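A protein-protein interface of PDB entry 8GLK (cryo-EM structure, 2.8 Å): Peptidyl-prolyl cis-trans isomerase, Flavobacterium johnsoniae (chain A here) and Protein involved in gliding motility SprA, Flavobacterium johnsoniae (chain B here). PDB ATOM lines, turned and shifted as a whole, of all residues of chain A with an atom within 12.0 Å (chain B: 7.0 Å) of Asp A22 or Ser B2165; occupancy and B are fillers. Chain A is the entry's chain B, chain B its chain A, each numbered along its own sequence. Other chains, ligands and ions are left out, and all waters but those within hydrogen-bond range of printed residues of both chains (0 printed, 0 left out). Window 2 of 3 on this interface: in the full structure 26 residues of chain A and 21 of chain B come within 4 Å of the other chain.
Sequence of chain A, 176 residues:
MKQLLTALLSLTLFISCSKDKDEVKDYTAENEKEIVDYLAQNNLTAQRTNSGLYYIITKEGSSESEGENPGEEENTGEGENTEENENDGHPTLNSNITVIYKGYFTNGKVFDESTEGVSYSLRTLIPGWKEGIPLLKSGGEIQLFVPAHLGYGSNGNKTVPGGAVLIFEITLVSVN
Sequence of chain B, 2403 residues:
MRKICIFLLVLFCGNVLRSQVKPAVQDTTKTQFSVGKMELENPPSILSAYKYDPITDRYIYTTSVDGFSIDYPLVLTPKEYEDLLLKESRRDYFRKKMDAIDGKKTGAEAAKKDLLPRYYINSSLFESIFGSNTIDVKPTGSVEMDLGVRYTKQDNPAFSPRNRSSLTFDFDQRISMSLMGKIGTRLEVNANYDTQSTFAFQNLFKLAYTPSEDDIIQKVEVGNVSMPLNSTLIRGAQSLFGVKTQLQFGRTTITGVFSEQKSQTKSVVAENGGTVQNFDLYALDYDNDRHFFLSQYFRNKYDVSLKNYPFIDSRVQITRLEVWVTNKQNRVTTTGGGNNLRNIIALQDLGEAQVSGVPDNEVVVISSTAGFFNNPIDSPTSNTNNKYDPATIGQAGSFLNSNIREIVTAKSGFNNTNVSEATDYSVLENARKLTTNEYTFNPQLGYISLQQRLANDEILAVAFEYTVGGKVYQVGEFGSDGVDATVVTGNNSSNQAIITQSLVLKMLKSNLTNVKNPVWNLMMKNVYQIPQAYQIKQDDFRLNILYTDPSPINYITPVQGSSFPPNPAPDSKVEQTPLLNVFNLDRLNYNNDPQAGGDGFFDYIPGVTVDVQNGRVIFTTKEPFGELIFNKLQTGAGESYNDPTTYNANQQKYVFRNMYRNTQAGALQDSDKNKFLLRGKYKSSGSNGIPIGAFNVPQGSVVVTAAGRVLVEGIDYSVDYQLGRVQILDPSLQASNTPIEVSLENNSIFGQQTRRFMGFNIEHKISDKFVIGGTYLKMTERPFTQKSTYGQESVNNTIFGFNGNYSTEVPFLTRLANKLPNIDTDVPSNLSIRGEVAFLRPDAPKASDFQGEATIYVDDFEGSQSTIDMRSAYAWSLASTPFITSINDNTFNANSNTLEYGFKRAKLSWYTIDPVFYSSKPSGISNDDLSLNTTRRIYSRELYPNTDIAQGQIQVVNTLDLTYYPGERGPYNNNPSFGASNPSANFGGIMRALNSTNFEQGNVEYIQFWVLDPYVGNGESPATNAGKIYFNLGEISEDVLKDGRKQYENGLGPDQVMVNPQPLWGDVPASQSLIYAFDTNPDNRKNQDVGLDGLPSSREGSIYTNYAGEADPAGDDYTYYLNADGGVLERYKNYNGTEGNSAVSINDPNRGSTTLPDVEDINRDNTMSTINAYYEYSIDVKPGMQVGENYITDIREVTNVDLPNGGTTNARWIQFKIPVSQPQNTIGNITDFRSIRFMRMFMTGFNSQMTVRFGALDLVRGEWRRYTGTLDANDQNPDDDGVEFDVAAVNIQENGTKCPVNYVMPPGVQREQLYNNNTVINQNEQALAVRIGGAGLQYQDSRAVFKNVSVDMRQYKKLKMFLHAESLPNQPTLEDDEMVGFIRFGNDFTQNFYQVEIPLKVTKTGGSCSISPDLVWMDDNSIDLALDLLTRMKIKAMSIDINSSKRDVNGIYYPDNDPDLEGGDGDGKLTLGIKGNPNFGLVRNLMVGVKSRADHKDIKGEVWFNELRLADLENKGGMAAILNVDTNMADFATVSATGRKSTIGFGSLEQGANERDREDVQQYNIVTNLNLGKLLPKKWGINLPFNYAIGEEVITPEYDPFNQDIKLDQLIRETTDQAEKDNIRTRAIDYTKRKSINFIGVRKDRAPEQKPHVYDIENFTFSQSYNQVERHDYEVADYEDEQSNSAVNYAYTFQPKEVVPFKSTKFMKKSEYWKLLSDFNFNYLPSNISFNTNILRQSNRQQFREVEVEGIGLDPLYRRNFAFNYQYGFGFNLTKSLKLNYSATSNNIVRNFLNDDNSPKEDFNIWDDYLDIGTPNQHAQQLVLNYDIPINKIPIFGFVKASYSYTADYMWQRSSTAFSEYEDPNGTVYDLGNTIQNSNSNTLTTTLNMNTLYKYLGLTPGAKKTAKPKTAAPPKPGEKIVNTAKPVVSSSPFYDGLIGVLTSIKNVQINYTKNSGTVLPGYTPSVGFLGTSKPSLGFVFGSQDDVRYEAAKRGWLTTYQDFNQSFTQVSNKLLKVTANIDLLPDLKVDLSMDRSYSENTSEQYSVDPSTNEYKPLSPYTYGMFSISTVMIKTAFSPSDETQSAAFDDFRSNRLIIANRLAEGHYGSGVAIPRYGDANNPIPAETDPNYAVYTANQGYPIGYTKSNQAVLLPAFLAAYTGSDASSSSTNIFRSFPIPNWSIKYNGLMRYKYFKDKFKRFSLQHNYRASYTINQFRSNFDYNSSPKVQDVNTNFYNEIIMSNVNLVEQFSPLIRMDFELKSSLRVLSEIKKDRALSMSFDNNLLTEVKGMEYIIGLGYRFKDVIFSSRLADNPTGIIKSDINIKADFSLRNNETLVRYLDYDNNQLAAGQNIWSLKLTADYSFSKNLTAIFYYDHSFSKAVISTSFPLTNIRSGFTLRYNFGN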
ATOM      1  N   ASP A  22     -15.359 -31.265  -7.676  1.00  0.00           N
ATOM      2  CA  ASP A  22     -16.801 -31.075  -7.792  1.00  0.00           C
ATOM      3  C   ASP A  22     -17.487 -31.304  -6.450  1.00  0.00           C
ATOM      4  O   ASP A  22     -17.868 -32.427  -6.118  1.00  0.00           O
ATOM      5  CB  ASP A  22     -17.380 -32.012  -8.853  1.00  0.00           C
ATOM      6  CG  ASP A  22     -16.911 -31.667 -10.253  1.00  0.00           C
ATOM      7  OD1 ASP A  22     -16.591 -30.485 -10.501  1.00  0.00           O
ATOM      8  OD2 ASP A  22     -16.859 -32.578 -11.107  1.00  0.00           O
ATOM      9  N   GLU A  23     -17.639 -30.229  -5.681  1.00  0.00           N
ATOM     10  CA  GLU A  23     -18.207 -30.269  -4.335  1.00  0.00           C
ATOM     11  C   GLU A  23     -19.225 -29.140  -4.179  1.00  0.00           C
ATOM     12  O   GLU A  23     -19.171 -28.324  -3.257  1.00  0.00           O
ATOM     13  CB  GLU A  23     -17.071 -30.223  -3.308  1.00  0.00           C
ATOM     14  CG  GLU A  23     -17.434 -30.633  -1.879  1.00  0.00           C
ATOM     15  CD  GLU A  23     -17.853 -29.475  -1.001  1.00  0.00           C
ATOM     16  OE1 GLU A  23     -17.349 -28.352  -1.211  1.00  0.00           O
ATOM     17  OE2 GLU A  23     -18.689 -29.686  -0.097  1.00  0.00           O
ATOM     18  N   VAL A  24     -20.161 -29.070  -5.127  1.00  0.00           N
ATOM     19  CA  VAL A  24     -21.091 -27.949  -5.198  1.00  0.00           C
ATOM     20  C   VAL A  24     -22.129 -28.037  -4.084  1.00  0.00           C
ATOM     21  O   VAL A  24     -22.297 -29.077  -3.431  1.00  0.00           O
ATOM     22  CB  VAL A  24     -21.767 -27.910  -6.580  1.00  0.00           C
ATOM     23  CG1 VAL A  24     -20.719 -27.878  -7.681  1.00  0.00           C
ATOM     24  CG2 VAL A  24     -22.696 -29.103  -6.751  1.00  0.00           C
ATOM     25  N   LYS A  25     -22.835 -26.928  -3.866  1.00  0.00           N
ATOM     26  CA  LYS A  25     -23.936 -26.840  -2.917  1.00  0.00           C
ATOM     27  C   LYS A  25     -25.203 -26.443  -3.660  1.00  0.00           C
ATOM     28  O   LYS A  25     -25.138 -25.911  -4.770  1.00  0.00           O
ATOM     29  CB  LYS A  25     -23.678 -25.801  -1.817  1.00  0.00           C
ATOM     30  CG  LYS A  25     -22.773 -26.219  -0.669  1.00  0.00           C
ATOM     31  CD  LYS A  25     -21.318 -26.285  -1.088  1.00  0.00           C
ATOM     32  CE  LYS A  25     -20.426 -26.607   0.098  1.00  0.00           C
ATOM     33  NZ  LYS A  25     -19.008 -26.787  -0.304  1.00  0.00           N
ATOM     34  N   ASP A  26     -26.355 -26.704  -3.047  1.00  0.00           N
ATOM     35  CA  ASP A  26     -27.636 -26.214  -3.542  1.00  0.00           C
ATOM     36  C   ASP A  26     -28.268 -25.319  -2.483  1.00  0.00           C
ATOM     37  O   ASP A  26     -28.301 -25.680  -1.301  1.00  0.00           O
ATOM     38  CB  ASP A  26     -28.571 -27.372  -3.893  1.00  0.00           C
ATOM     39  CG  ASP A  26     -29.840 -26.908  -4.584  1.00  0.00           C
ATOM     40  OD1 ASP A  26     -29.931 -25.713  -4.933  1.00  0.00           O
ATOM     41  OD2 ASP A  26     -30.749 -27.742  -4.781  1.00  0.00           O
ATOM     42  N   SER A 154     -23.187 -19.696  -5.344  1.00  0.00           N
ATOM     43  CA  SER A 154     -22.992 -20.565  -4.192  1.00  0.00           C
ATOM     44  C   SER A 154     -21.601 -20.452  -3.586  1.00  0.00           C
ATOM     45  O   SER A 154     -21.356 -21.040  -2.527  1.00  0.00           O
ATOM     46  CB  SER A 154     -23.264 -22.020  -4.581  1.00  0.00           C
ATOM     47  OG  SER A 154     -24.585 -22.175  -5.071  1.00  0.00           O
ATOM     48  N   ASN A 155     -20.687 -19.725  -4.224  1.00  0.00           N
ATOM     49  CA  ASN A 155     -19.348 -19.528  -3.683  1.00  0.00           C
ATOM     50  C   ASN A 155     -19.134 -18.138  -3.107  1.00  0.00           C
ATOM     51  O   ASN A 155     -18.284 -17.971  -2.226  1.00  0.00           O
ATOM     52  CB  ASN A 155     -18.295 -19.790  -4.765  1.00  0.00           C
ATOM     53  CG  ASN A 155     -18.648 -19.147  -6.092  1.00  0.00           C
ATOM     54  OD1 ASN A 155     -19.585 -18.352  -6.179  1.00  0.00           O
ATOM     55  ND2 ASN A 155     -17.897 -19.486  -7.132  1.00  0.00           N
ATOM     56  N   ASN B2093     -10.830 -28.722 -23.549  1.00  0.00           N
ATOM     57  CA  ASN B2093     -11.017 -28.613 -22.106  1.00  0.00           C
ATOM     58  C   ASN B2093     -11.711 -27.327 -21.684  1.00  0.00           C
ATOM     59  O   ASN B2093     -12.139 -27.231 -20.527  1.00  0.00           O
ATOM     60  CB  ASN B2093      -9.667 -28.712 -21.392  1.00  0.00           C
ATOM     61  CG  ASN B2093      -9.046 -30.087 -21.507  1.00  0.00           C
ATOM     62  OD1 ASN B2093      -9.711 -31.052 -21.881  1.00  0.00           O
ATOM     63  ND2 ASN B2093      -7.764 -30.185 -21.181  1.00  0.00           N
ATOM     64  N   ILE B2096     -15.359 -28.011 -20.682  1.00  0.00           N
ATOM     65  CA  ILE B2096     -15.434 -28.804 -19.457  1.00  0.00           C
ATOM     66  C   ILE B2096     -15.140 -27.932 -18.243  1.00  0.00           C
ATOM     67  O   ILE B2096     -15.855 -27.974 -17.231  1.00  0.00           O
ATOM     68  CB  ILE B2096     -14.475 -30.005 -19.536  1.00  0.00           C
ATOM     69  CG1 ILE B2096     -14.768 -30.837 -20.785  1.00  0.00           C
ATOM     70  CG2 ILE B2096     -14.582 -30.857 -18.283  1.00  0.00           C
ATOM     71  CD1 ILE B2096     -13.739 -31.908 -21.056  1.00  0.00           C
ATOM     72  N   ILE B2097     -14.082 -27.121 -18.328  1.00  0.00           N
ATOM     73  CA  ILE B2097     -13.734 -26.241 -17.219  1.00  0.00           C
ATOM     74  C   ILE B2097     -14.822 -25.198 -16.999  1.00  0.00           C
ATOM     75  O   ILE B2097     -15.154 -24.863 -15.856  1.00  0.00           O
ATOM     76  CB  ILE B2097     -12.361 -25.591 -17.463  1.00  0.00           C
ATOM     77  CG1 ILE B2097     -11.267 -26.660 -17.497  1.00  0.00           C
ATOM     78  CG2 ILE B2097     -12.063 -24.562 -16.390  1.00  0.00           C
ATOM     79  CD1 ILE B2097     -11.125 -27.429 -16.205  1.00  0.00           C
ATOM     80  N   ASN B2099     -18.034 -25.541 -17.626  1.00  0.00           N
ATOM     81  CA  ASN B2099     -19.164 -26.205 -16.985  1.00  0.00           C
ATOM     82  C   ASN B2099     -18.893 -26.457 -15.506  1.00  0.00           C
ATOM     83  O   ASN B2099     -19.783 -26.269 -14.666  1.00  0.00           O
ATOM     84  CB  ASN B2099     -19.483 -27.514 -17.705  1.00  0.00           C
ATOM     85  CG  ASN B2099     -20.312 -27.302 -18.955  1.00  0.00           C
ATOM     86  OD1 ASN B2099     -21.126 -26.384 -19.024  1.00  0.00           O
ATOM     87  ND2 ASN B2099     -20.108 -28.155 -19.951  1.00  0.00           N
ATOM     88  N   ARG B2100     -17.673 -26.885 -15.169  1.00  0.00           N
ATOM     89  CA  ARG B2100     -17.336 -27.087 -13.762  1.00  0.00           C
ATOM     90  C   ARG B2100     -17.419 -25.781 -12.981  1.00  0.00           C
ATOM     91  O   ARG B2100     -17.961 -25.744 -11.869  1.00  0.00           O
ATOM     92  CB  ARG B2100     -15.940 -27.698 -13.636  1.00  0.00           C
ATOM     93  CG  ARG B2100     -15.848 -29.138 -14.108  1.00  0.00           C
ATOM     94  CD  ARG B2100     -14.424 -29.654 -14.008  1.00  0.00           C
ATOM     95  NE  ARG B2100     -13.911 -29.572 -12.646  1.00  0.00           N
ATOM     96  CZ  ARG B2100     -12.626 -29.635 -12.324  1.00  0.00           C
ATOM     97  NH1 ARG B2100     -11.689 -29.776 -13.247  1.00  0.00           N
ATOM     98  NH2 ARG B2100     -12.273 -29.554 -11.045  1.00  0.00           N
ATOM     99  N   LEU B2101     -16.903 -24.693 -13.555  1.00  0.00           N
ATOM    100  CA  LEU B2101     -16.950 -23.401 -12.879  1.00  0.00           C
ATOM    101  C   LEU B2101     -18.380 -22.895 -12.745  1.00  0.00           C
ATOM    102  O   LEU B2101     -18.727 -22.263 -11.741  1.00  0.00           O
ATOM    103  CB  LEU B2101     -16.089 -22.386 -13.628  1.00  0.00           C
ATOM    104  CG  LEU B2101     -14.578 -22.613 -13.573  1.00  0.00           C
ATOM    105  CD1 LEU B2101     -13.849 -21.511 -14.318  1.00  0.00           C
ATOM    106  CD2 LEU B2101     -14.101 -22.696 -12.133  1.00  0.00           C
ATOM    107  N   GLU B2103     -21.091 -24.832 -12.483  1.00  0.00           N
ATOM    108  CA  GLU B2103     -21.686 -25.616 -11.406  1.00  0.00           C
ATOM    109  C   GLU B2103     -21.193 -25.137 -10.047  1.00  0.00           C
ATOM    110  O   GLU B2103     -21.938 -25.164  -9.061  1.00  0.00           O
ATOM    111  CB  GLU B2103     -21.382 -27.100 -11.604  1.00  0.00           C
ATOM    112  CG  GLU B2103     -22.430 -27.835 -12.426  1.00  0.00           C
ATOM    113  CD  GLU B2103     -22.036 -29.266 -12.732  1.00  0.00           C
ATOM    114  OE1 GLU B2103     -22.104 -30.112 -11.816  1.00  0.00           O
ATOM    115  OE2 GLU B2103     -21.661 -29.545 -13.891  1.00  0.00           O
ATOM    116  N   GLY B2104     -19.934 -24.702  -9.974  1.00  0.00           N
ATOM    117  CA  GLY B2104     -19.447 -24.089  -8.749  1.00  0.00           C
ATOM    118  C   GLY B2104     -20.135 -22.772  -8.439  1.00  0.00           C
ATOM    119  O   GLY B2104     -20.365 -22.442  -7.272  1.00  0.00           O
ATOM    120  N   ALA B2157      -4.273 -28.480 -17.558  1.00  0.00           N
ATOM    121  CA  ALA B2157      -4.709 -29.865 -17.696  1.00  0.00           C
ATOM    122  C   ALA B2157      -4.303 -30.444 -19.043  1.00  0.00           C
ATOM    123  O   ALA B2157      -3.908 -31.613 -19.128  1.00  0.00           O
ATOM    124  CB  ALA B2157      -6.222 -29.959 -17.505  1.00  0.00           C
ATOM    125  N   SER B2162      -3.387 -34.137 -17.614  1.00  0.00           N
ATOM    126  CA  SER B2162      -4.464 -34.414 -16.680  1.00  0.00           C
ATOM    127  C   SER B2162      -5.819 -34.363 -17.384  1.00  0.00           C
ATOM    128  O   SER B2162      -5.948 -33.911 -18.525  1.00  0.00           O
ATOM    129  CB  SER B2162      -4.432 -33.424 -15.518  1.00  0.00           C
ATOM    130  OG  SER B2162      -3.171 -33.436 -14.873  1.00  0.00           O
ATOM    131  N   ASP B2163      -6.842 -34.838 -16.679  1.00  0.00           N
ATOM    132  CA  ASP B2163      -8.205 -34.846 -17.192  1.00  0.00           C
ATOM    133  C   ASP B2163      -8.953 -33.627 -16.670  1.00  0.00           C
ATOM    134  O   ASP B2163      -8.994 -33.388 -15.459  1.00  0.00           O
ATOM    135  CB  ASP B2163      -8.925 -36.130 -16.781  1.00  0.00           C
ATOM    136  CG  ASP B2163     -10.232 -36.328 -17.521  1.00  0.00           C
ATOM    137  OD1 ASP B2163     -10.207 -36.398 -18.768  1.00  0.00           O
ATOM    138  OD2 ASP B2163     -11.284 -36.418 -16.856  1.00  0.00           O
ATOM    139  N   ALA B2164      -9.544 -32.858 -17.589  1.00  0.00           N
ATOM    140  CA  ALA B2164     -10.209 -31.616 -17.215  1.00  0.00           C
ATOM    141  C   ALA B2164     -11.428 -31.842 -16.330  1.00  0.00           C
ATOM    142  O   ALA B2164     -11.849 -30.913 -15.633  1.00  0.00           O
ATOM    143  CB  ALA B2164     -10.616 -30.839 -18.466  1.00  0.00           C
ATOM    144  N   SER B2165     -12.005 -33.045 -16.343  1.00  0.00           N
ATOM    145  CA  SER B2165     -13.163 -33.319 -15.501  1.00  0.00           C
ATOM    146  C   SER B2165     -12.809 -33.361 -14.021  1.00  0.00           C
ATOM    147  O   SER B2165     -13.697 -33.195 -13.180  1.00  0.00           O
ATOM    148  CB  SER B2165     -13.816 -34.639 -15.917  1.00  0.00           C
ATOM    149  OG  SER B2165     -14.243 -34.593 -17.266  1.00  0.00           O
ATOM    150  N   SER B2166     -11.536 -33.579 -13.685  1.00  0.00           N
ATOM    151  CA  SER B2166     -11.117 -33.636 -12.293  1.00  0.00           C
ATOM    152  C   SER B2166      -9.845 -32.851 -12.005  1.00  0.00           C
ATOM    153  O   SER B2166      -9.362 -32.896 -10.869  1.00  0.00           O
ATOM    154  CB  SER B2166     -10.920 -35.095 -11.852  1.00  0.00           C
ATOM    155  OG  SER B2166      -9.930 -35.735 -12.639  1.00  0.00           O
ATOM    156  N   SER B2167      -9.288 -32.141 -12.981  1.00  0.00           N
ATOM    157  CA  SER B2167      -8.077 -31.373 -12.748  1.00  0.00           C
ATOM    158  C   SER B2167      -8.368 -30.165 -11.862  1.00  0.00           C
ATOM    159  O   SER B2167      -9.507 -29.706 -11.741  1.00  0.00           O
ATOM    160  CB  SER B2167      -7.465 -30.917 -14.072  1.00  0.00           C
ATOM    161  OG  SER B2167      -8.312 -29.995 -14.732  1.00  0.00           O
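NE of Arg B2100 is in salt-bridge range of OD1 of Asp A22 (3.6 Å).
NH1 of Arg B2100 sits at hydrogen-bond distance from O of Ser B2167, 2.7 Å away.
O of Ala B2164 is in hydrogen-bond range of NH1 of Arg B2100.
The backbone NH (N) of Ser B2165 lies close to the side-chain carboxylate (OD2) of Asp B2163, at 3.5 Å.
O of Ser B2165 touches OD2 of Asp A22 (3.8 Å).
O of Glu B2103 touches CG1 of Val A24 (3.3 Å).
CG1 of Val A24 touches N of Gly B2104 (3.995 Å).
CB of Ser A154 touches O of Gly B2104 (3.98 Å).
Asn A155 touches Gly B2104.
Asp A22 touches just these residues of chain B: Arg B2100 and Ser B2165.
Arg B2100 touches one residue of chain A.
No residue of chain A comes within 4 Å of Ala B2164.
No residue of chain A comes within 4 Å of Ser B2166.
No residue of chain A comes within 4 Å of Ser B2167.
Printed residues of chain A within 4 Å of Gly B2104: Val A24, Ser A154 and Asn A155.
Printed residues of chain B within 4 Å of Val A24: Glu B2103 and Gly B2104.
The nearest residue of chain A that does not touch Ser B2165 is Glu A23 (9.0 Å).
The nearest printed residue of chain A that does not touch Gly B2104 is Lys A25 (6.2 Å).
Printed residues of chain B that touch a printed residue of chain A: Arg B2100, Glu B2103, Gly B2104 and Ser B2165.
Along chain B the printed residues that touch a printed residue of chain A span positions 2100 to 2165.
Of the 7 printed residues of chain A, 4 touch a printed residue of chain B.
Hydrophobic or aromatic side chains of chain A within 4 Å of the printed part of chain B: Val A24.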
